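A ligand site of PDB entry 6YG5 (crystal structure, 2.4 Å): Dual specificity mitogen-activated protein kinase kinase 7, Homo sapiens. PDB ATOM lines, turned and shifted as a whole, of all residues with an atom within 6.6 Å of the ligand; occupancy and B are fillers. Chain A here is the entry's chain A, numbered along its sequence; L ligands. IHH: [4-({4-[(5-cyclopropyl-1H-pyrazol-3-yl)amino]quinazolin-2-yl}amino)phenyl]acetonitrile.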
ATOM      1  N   MET A  28       9.565   4.130 -11.746  1.00  0.00           N
ATOM      2  CA  MET A  28       8.816   4.992 -10.796  1.00  0.00           C
ATOM      3  C   MET A  28       9.803   5.887 -10.015  1.00  0.00           C
ATOM      4  O   MET A  28       9.476   7.066  -9.798  1.00  0.00           O
ATOM      5  CB  MET A  28       7.992   4.154  -9.832  1.00  0.00           C
ATOM      6  CG  MET A  28       6.723   3.622 -10.442  1.00  0.00           C
ATOM      7  SD  MET A  28       5.717   2.677  -9.289  1.00  0.00           S
ATOM      8  CE  MET A  28       6.964   1.785  -8.379  1.00  0.00           C
ATOM      9  N   GLY A  29      10.969   5.338  -9.652  1.00  0.00           N
ATOM     10  CA  GLY A  29      12.022   6.040  -8.873  1.00  0.00           C
ATOM     11  C   GLY A  29      13.178   5.111  -8.524  1.00  0.00           C
ATOM     12  O   GLY A  29      13.086   4.452  -7.464  1.00  0.00           O
ATOM     13  N   GLY A  34      17.193   3.077  -6.837  1.00  0.00           N
ATOM     14  CA  GLY A  34      16.865   1.634  -6.812  1.00  0.00           C
ATOM     15  C   GLY A  34      15.779   1.284  -7.819  1.00  0.00           C
ATOM     16  O   GLY A  34      14.635   1.822  -7.676  1.00  0.00           O
ATOM     17  N   VAL A  36      12.937   0.310  -9.526  1.00  0.00           N
ATOM     18  CA  VAL A  36      11.537  -0.191  -9.350  1.00  0.00           C
ATOM     19  C   VAL A  36      10.664   0.239 -10.545  1.00  0.00           C
ATOM     20  O   VAL A  36      10.470   1.445 -10.745  1.00  0.00           O
ATOM     21  CB  VAL A  36      10.919   0.268  -8.017  1.00  0.00           C
ATOM     22  CG1 VAL A  36      10.963   1.780  -7.869  1.00  0.00           C
ATOM     23  CG2 VAL A  36       9.506  -0.260  -7.839  1.00  0.00           C
ATOM     24  N   ALA A  49       4.023  -2.968  -9.097  1.00  0.00           N
ATOM     25  CA  ALA A  49       5.401  -2.502  -8.959  1.00  0.00           C
ATOM     26  C   ALA A  49       6.327  -3.722  -8.996  1.00  0.00           C
ATOM     27  O   ALA A  49       5.892  -4.810  -8.572  1.00  0.00           O
ATOM     28  CB  ALA A  49       5.554  -1.715  -7.685  1.00  0.00           C
ATOM     29  N   VAL A  50       7.498  -3.559  -9.592  1.00  0.00           N
ATOM     30  CA  VAL A  50       8.456  -4.652  -9.854  1.00  0.00           C
ATOM     31  C   VAL A  50       9.850  -4.128  -9.570  1.00  0.00           C
ATOM     32  O   VAL A  50      10.303  -3.193 -10.278  1.00  0.00           O
ATOM     33  CB  VAL A  50       8.321  -5.188 -11.281  1.00  0.00           C
ATOM     34  CG1 VAL A  50       9.399  -6.202 -11.607  1.00  0.00           C
ATOM     35  CG2 VAL A  50       6.961  -5.794 -11.510  1.00  0.00           C
ATOM     36  N   LYS A  51      10.482  -4.657  -8.517  1.00  0.00           N
ATOM     37  CA  LYS A  51      11.913  -4.411  -8.226  1.00  0.00           C
ATOM     38  C   LYS A  51      12.723  -5.451  -8.993  1.00  0.00           C
ATOM     39  O   LYS A  51      12.359  -6.637  -8.956  1.00  0.00           O
ATOM     40  CB  LYS A  51      12.149  -4.442  -6.723  1.00  0.00           C
ATOM     41  CG  LYS A  51      11.235  -3.495  -5.952  1.00  0.00           C
ATOM     42  N   ASP A  68      15.300  -6.961   3.079  1.00  0.00           N
ATOM     43  CA  ASP A  68      14.042  -6.200   2.965  1.00  0.00           C
ATOM     44  C   ASP A  68      12.925  -7.143   2.474  1.00  0.00           C
ATOM     45  O   ASP A  68      11.836  -7.090   3.051  1.00  0.00           O
ATOM     46  CB  ASP A  68      14.257  -4.959   2.103  1.00  0.00           C
ATOM     47  CG  ASP A  68      15.073  -3.868   2.796  1.00  0.00           C
ATOM     48  OD1 ASP A  68      15.342  -3.991   4.044  1.00  0.00           O
ATOM     49  OD2 ASP A  68      15.412  -2.861   2.101  1.00  0.00           O
ATOM     50  N   VAL A  82       3.473  -2.925   2.689  1.00  0.00           N
ATOM     51  CA  VAL A  82       3.295  -3.291   1.258  1.00  0.00           C
ATOM     52  C   VAL A  82       3.577  -4.782   1.111  1.00  0.00           C
ATOM     53  O   VAL A  82       4.600  -5.245   1.640  1.00  0.00           O
ATOM     54  CB  VAL A  82       4.172  -2.446   0.323  1.00  0.00           C
ATOM     55  CG1 VAL A  82       3.673  -1.029   0.213  1.00  0.00           C
ATOM     56  CG2 VAL A  82       5.638  -2.458   0.733  1.00  0.00           C
ATOM     57  N   MET A  98       5.539  -6.381  -6.318  1.00  0.00           N
ATOM     58  CA  MET A  98       5.009  -5.662  -5.141  1.00  0.00           C
ATOM     59  C   MET A  98       3.661  -5.007  -5.501  1.00  0.00           C
ATOM     60  O   MET A  98       3.515  -4.477  -6.617  1.00  0.00           O
ATOM     61  CB  MET A  98       5.976  -4.575  -4.669  1.00  0.00           C
ATOM     62  CG  MET A  98       7.367  -5.092  -4.266  1.00  0.00           C
ATOM     63  SD  MET A  98       7.298  -6.120  -2.810  1.00  0.00           S
ATOM     64  CE  MET A  98       6.880  -4.912  -1.546  1.00  0.00           C
ATOM     65  N   GLU A  99       2.758  -4.980  -4.555  1.00  0.00           N
ATOM     66  CA  GLU A  99       1.642  -4.018  -4.444  1.00  0.00           C
ATOM     67  C   GLU A  99       2.088  -2.648  -4.961  1.00  0.00           C
ATOM     68  O   GLU A  99       3.082  -2.114  -4.448  1.00  0.00           O
ATOM     69  CB  GLU A  99       1.237  -3.955  -2.977  1.00  0.00           C
ATOM     70  CG  GLU A  99      -0.083  -3.295  -2.723  1.00  0.00           C
ATOM     71  CD  GLU A  99      -0.600  -3.516  -1.317  1.00  0.00           C
ATOM     72  OE1 GLU A  99       0.129  -4.134  -0.510  1.00  0.00           O
ATOM     73  OE2 GLU A  99      -1.737  -3.085  -1.026  1.00  0.00           O
ATOM     74  N   LEU A 100       1.373  -2.082  -5.932  1.00  0.00           N
ATOM     75  CA  LEU A 100       1.603  -0.713  -6.464  1.00  0.00           C
ATOM     76  C   LEU A 100       0.808   0.279  -5.621  1.00  0.00           C
ATOM     77  O   LEU A 100      -0.421   0.081  -5.486  1.00  0.00           O
ATOM     78  CB  LEU A 100       1.180  -0.639  -7.940  1.00  0.00           C
ATOM     79  CG  LEU A 100       1.389   0.708  -8.631  1.00  0.00           C
ATOM     80  CD1 LEU A 100       2.834   1.145  -8.564  1.00  0.00           C
ATOM     81  CD2 LEU A 100       0.967   0.649 -10.057  1.00  0.00           C
ATOM     82  N   MET A 101       1.477   1.320  -5.127  1.00  0.00           N
ATOM     83  CA  MET A 101       0.844   2.455  -4.418  1.00  0.00           C
ATOM     84  C   MET A 101       1.027   3.737  -5.263  1.00  0.00           C
ATOM     85  O   MET A 101       1.907   3.749  -6.139  1.00  0.00           O
ATOM     86  CB  MET A 101       1.475   2.650  -3.035  1.00  0.00           C
ATOM     87  CG  MET A 101       1.623   1.351  -2.248  1.00  0.00           C
ATOM     88  SD  MET A 101       0.093   0.826  -1.431  1.00  0.00           S
ATOM     89  CE  MET A 101      -0.063   2.100  -0.176  1.00  0.00           C
ATOM     90  N   GLY A 102       0.215   4.756  -4.986  1.00  0.00           N
ATOM     91  CA  GLY A 102       0.146   6.002  -5.774  1.00  0.00           C
ATOM     92  C   GLY A 102       1.382   6.861  -5.612  1.00  0.00           C
ATOM     93  O   GLY A 102       1.845   7.409  -6.621  1.00  0.00           O
ATOM     94  N   THR A 103       1.899   7.026  -4.382  1.00  0.00           N
ATOM     95  CA  THR A 103       3.010   7.968  -4.102  1.00  0.00           C
ATOM     96  C   THR A 103       3.534   7.759  -2.682  1.00  0.00           C
ATOM     97  O   THR A 103       2.919   7.013  -1.915  1.00  0.00           O
ATOM     98  CB  THR A 103       2.552   9.409  -4.362  1.00  0.00           C
ATOM     99  OG1 THR A 103       3.655  10.295  -4.162  1.00  0.00           O
ATOM    100  CG2 THR A 103       1.403   9.831  -3.483  1.00  0.00           C
ATOM    101  N   CSO A 104       4.671   8.361  -2.381  1.00  0.00           N
ATOM    102  CA  CSO A 104       5.227   8.458  -1.025  1.00  0.00           C
ATOM    103  CB  CSO A 104       6.681   8.173  -1.054  1.00  0.00           C
ATOM    104  SG  CSO A 104       7.630   9.451  -1.892  1.00  0.00           S
ATOM    105  C   CSO A 104       4.938   9.845  -0.471  1.00  0.00           C
ATOM    106  O   CSO A 104       4.580  10.733  -1.280  1.00  0.00           O
ATOM    107  OD  CSO A 104       8.980   8.695  -2.495  1.00  0.00           O
ATOM    108  N   LYS A 107       6.946  12.959  -1.911  1.00  0.00           N
ATOM    109  CA  LYS A 107       6.453  13.350  -3.246  1.00  0.00           C
ATOM    110  C   LYS A 107       5.067  13.982  -3.079  1.00  0.00           C
ATOM    111  O   LYS A 107       4.723  14.897  -3.889  1.00  0.00           O
ATOM    112  CB  LYS A 107       6.387  12.135  -4.177  1.00  0.00           C
ATOM    113  CG  LYS A 107       7.737  11.664  -4.724  1.00  0.00           C
ATOM    114  CD  LYS A 107       7.628  10.918  -6.062  1.00  0.00           C
ATOM    115  CE  LYS A 107       8.948  10.344  -6.533  1.00  0.00           C
ATOM    116  NZ  LYS A 107       9.480   9.331  -5.573  1.00  0.00           N
ATOM    117  N   SER A 149       9.476   9.584   2.710  1.00  0.00           N
ATOM    118  CA  SER A 149       9.763   8.818   1.464  1.00  0.00           C
ATOM    119  C   SER A 149       9.463   7.328   1.675  1.00  0.00           C
ATOM    120  O   SER A 149       9.256   6.632   0.668  1.00  0.00           O
ATOM    121  CB  SER A 149      11.165   9.039   1.006  1.00  0.00           C
ATOM    122  OG  SER A 149      12.072   8.244   1.748  1.00  0.00           O
ATOM    123  N   LEU A 152       3.838   5.324   2.192  1.00  0.00           N
ATOM    124  CA  LEU A 152       3.156   5.161   0.883  1.00  0.00           C
ATOM    125  C   LEU A 152       1.660   5.310   1.071  1.00  0.00           C
ATOM    126  O   LEU A 152       1.137   4.746   2.065  1.00  0.00           O
ATOM    127  CB  LEU A 152       3.496   3.791   0.291  1.00  0.00           C
ATOM    128  CG  LEU A 152       4.949   3.601  -0.166  1.00  0.00           C
ATOM    129  CD1 LEU A 152       5.102   2.273  -0.897  1.00  0.00           C
ATOM    130  CD2 LEU A 152       5.407   4.748  -1.052  1.00  0.00           C
ATOM    131  N   LEU A 153       0.998   6.021   0.151  1.00  0.00           N
ATOM    132  CA  LEU A 153      -0.470   6.159   0.070  1.00  0.00           C
ATOM    133  C   LEU A 153      -0.951   5.706  -1.298  1.00  0.00           C
ATOM    134  O   LEU A 153      -0.142   5.727  -2.260  1.00  0.00           O
ATOM    135  CB  LEU A 153      -0.845   7.604   0.332  1.00  0.00           C
ATOM    136  CG  LEU A 153      -0.240   8.199   1.589  1.00  0.00           C
ATOM    137  CD1 LEU A 153       1.040   8.933   1.255  1.00  0.00           C
ATOM    138  CD2 LEU A 153      -1.222   9.121   2.287  1.00  0.00           C
ATOM    139  N   CSO A 162       6.873   1.361   3.710  1.00  0.00           N
ATOM    140  CA  CSO A 162       7.559   0.952   2.468  1.00  0.00           C
ATOM    141  CB  CSO A 162       8.075   2.144   1.701  1.00  0.00           C
ATOM    142  SG  CSO A 162       9.029   1.694   0.242  1.00  0.00           S
ATOM    143  C   CSO A 162       8.700  -0.015   2.805  1.00  0.00           C
ATOM    144  O   CSO A 162       9.395   0.255   3.788  1.00  0.00           O
ATOM    145  OD  CSO A 162       9.924   2.947  -0.391  1.00  0.00           O
ATOM    146  N   ASP A 163       8.995  -0.922   1.865  1.00  0.00           N
ATOM    147  CA  ASP A 163       9.729  -2.197   2.037  1.00  0.00           C
ATOM    148  C   ASP A 163      11.240  -1.923   2.025  1.00  0.00           C
ATOM    149  O   ASP A 163      12.032  -2.913   2.183  1.00  0.00           O
ATOM    150  CB  ASP A 163       9.305  -3.224   0.972  1.00  0.00           C
ATOM    151  CG  ASP A 163       9.950  -3.044  -0.413  1.00  0.00           C
ATOM    152  OD1 ASP A 163      10.138  -1.884  -0.839  1.00  0.00           O
ATOM    153  OD2 ASP A 163      10.234  -4.084  -1.058  1.00  0.00           O
ATOM    154  N   PHE A 164      11.620  -0.652   1.868  1.00  0.00           N
ATOM    155  CA  PHE A 164      13.010  -0.164   1.932  1.00  0.00           C
ATOM    156  C   PHE A 164      13.494  -0.215   3.379  1.00  0.00           C
ATOM    157  O   PHE A 164      12.665  -0.046   4.315  1.00  0.00           O
ATOM    158  CB  PHE A 164      13.110   1.261   1.385  1.00  0.00           C
ATOM    159  CG  PHE A 164      14.521   1.751   1.140  1.00  0.00           C
ATOM    160  CD1 PHE A 164      15.424   0.983   0.419  1.00  0.00           C
ATOM    161  CD2 PHE A 164      14.933   2.992   1.610  1.00  0.00           C
ATOM    162  CE1 PHE A 164      16.720   1.444   0.189  1.00  0.00           C
ATOM    163  CE2 PHE A 164      16.224   3.456   1.372  1.00  0.00           C
ATOM    164  CZ  PHE A 164      17.110   2.674   0.657  1.00  0.00           C
ATOM    165  N   MET A 300      -3.724  14.585  -6.241  1.00  0.00           N
ATOM    166  CA  MET A 300      -2.938  13.977  -7.341  1.00  0.00           C
ATOM    167  C   MET A 300      -3.479  14.494  -8.689  1.00  0.00           C
ATOM    168  O   MET A 300      -2.681  14.645  -9.637  1.00  0.00           O
ATOM    169  CB  MET A 300      -3.012  12.447  -7.310  1.00  0.00           C
ATOM    170  CG  MET A 300      -2.374  11.847  -6.099  1.00  0.00           C
ATOM    171  SD  MET A 300      -0.564  12.034  -6.084  1.00  0.00           S
ATOM    172  CE  MET A 300      -0.109  10.947  -7.448  1.00  0.00           C
HETATM  173  C3  IHH L   1       5.344   7.865  -6.986  1.00  0.00           C
HETATM  174  C5  IHH L   1       4.910   5.555  -6.073  1.00  0.00           C
HETATM  175  C6  IHH L   1       5.788   6.595  -6.320  1.00  0.00           C
HETATM  176  C8  IHH L   1       7.495   5.321  -5.491  1.00  0.00           C
HETATM  177  C10 IHH L   1       5.420   4.389  -5.529  1.00  0.00           C
HETATM  178  C12 IHH L   1       9.701   4.272  -4.678  1.00  0.00           C
HETATM  179  C13 IHH L   1       9.275   3.263  -3.837  1.00  0.00           C
HETATM  180  C14 IHH L   1      10.176   2.330  -3.350  1.00  0.00           C
HETATM  181  C15 IHH L   1      11.518   2.386  -3.705  1.00  0.00           C
HETATM  182  C28 IHH L   1       8.119  -0.983  -4.209  1.00  0.00           C
HETATM  183  C29 IHH L   1       7.882  -0.617  -2.804  1.00  0.00           C
HETATM  184  C27 IHH L   1       6.714  -0.949  -3.676  1.00  0.00           C
HETATM  185  C24 IHH L   1       5.839   0.134  -4.095  1.00  0.00           C
HETATM  186  C23 IHH L   1       6.133   1.437  -4.431  1.00  0.00           C
HETATM  187  N25 IHH L   1       4.506   0.005  -4.249  1.00  0.00           N
HETATM  188  N26 IHH L   1       3.906   1.147  -4.675  1.00  0.00           N
HETATM  189  C22 IHH L   1       4.911   2.005  -4.791  1.00  0.00           C
HETATM  190  N21 IHH L   1       4.601   3.274  -5.275  1.00  0.00           N
HETATM  191  N9  IHH L   1       6.718   4.264  -5.225  1.00  0.00           N
HETATM  192  N7  IHH L   1       7.094   6.499  -6.026  1.00  0.00           N
HETATM  193  N11 IHH L   1       8.844   5.219  -5.283  1.00  0.00           N
HETATM  194  C17 IHH L   1      11.037   4.330  -5.041  1.00  0.00           C
HETATM  195  C16 IHH L   1      11.933   3.399  -4.563  1.00  0.00           C
HETATM  196  C18 IHH L   1      12.542   1.417  -3.133  1.00  0.00           C
HETATM  197  C19 IHH L   1      12.076   0.036  -3.083  1.00  0.00           C
HETATM  198  N20 IHH L   1      11.751  -1.057  -3.046  1.00  0.00           N
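N of Met 101 sits at hydrogen-bond distance from N26 of the ligand, 2.5 Å away.
O of Met 101 lies within hydrogen-bond range of N21 of the ligand, 2.9 Å away.
O of Glu 99 is in hydrogen-bond range of N25 of the ligand, at 2.6 Å.
A nitrogen (N20) of the ligand sits at hydrogen-bond distance from the side-chain carboxylate (OD1) of Asp 163 (2.9 Å).
The backbone NH (N) of Gly 102 lies within hydrogen-bond range of the backbone carbonyl oxygen (O) of Leu 153 (2.9 Å).
The backbone NH of Leu 153 sits at hydrogen-bond distance from the backbone carbonyl oxygen of Thr 103 (3.0 Å).
NZ of Lys 107 lies within hydrogen-bond range of OD of CSO 104 (3.2 Å).
O of Val 36 is in hydrogen-bond range of N of Met 28 (3.0 Å).
O of Ala 49 is in hydrogen-bond range of N of Met 98 (2.8 Å).
Merely in contact with the ligand: Gly 29, Val 36, Ala 49, Lys 51, Met 98, Leu 100, Gly 102, Thr 103, Lys 107, Leu 152 and CSO 162.
Hydrophobic or aromatic side chains within 4 Å of the ligand: Val 36, Ala 49, Met 98, Met 101 and Leu 152.
Within 4 Å of the ligand: Gly 29, Val 36, Ala 49, Lys 51, Met 98, Glu 99, Leu 100, Met 101, Gly 102, Thr 103, Lys 107, Leu 152, CSO 162 and Asp 163.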
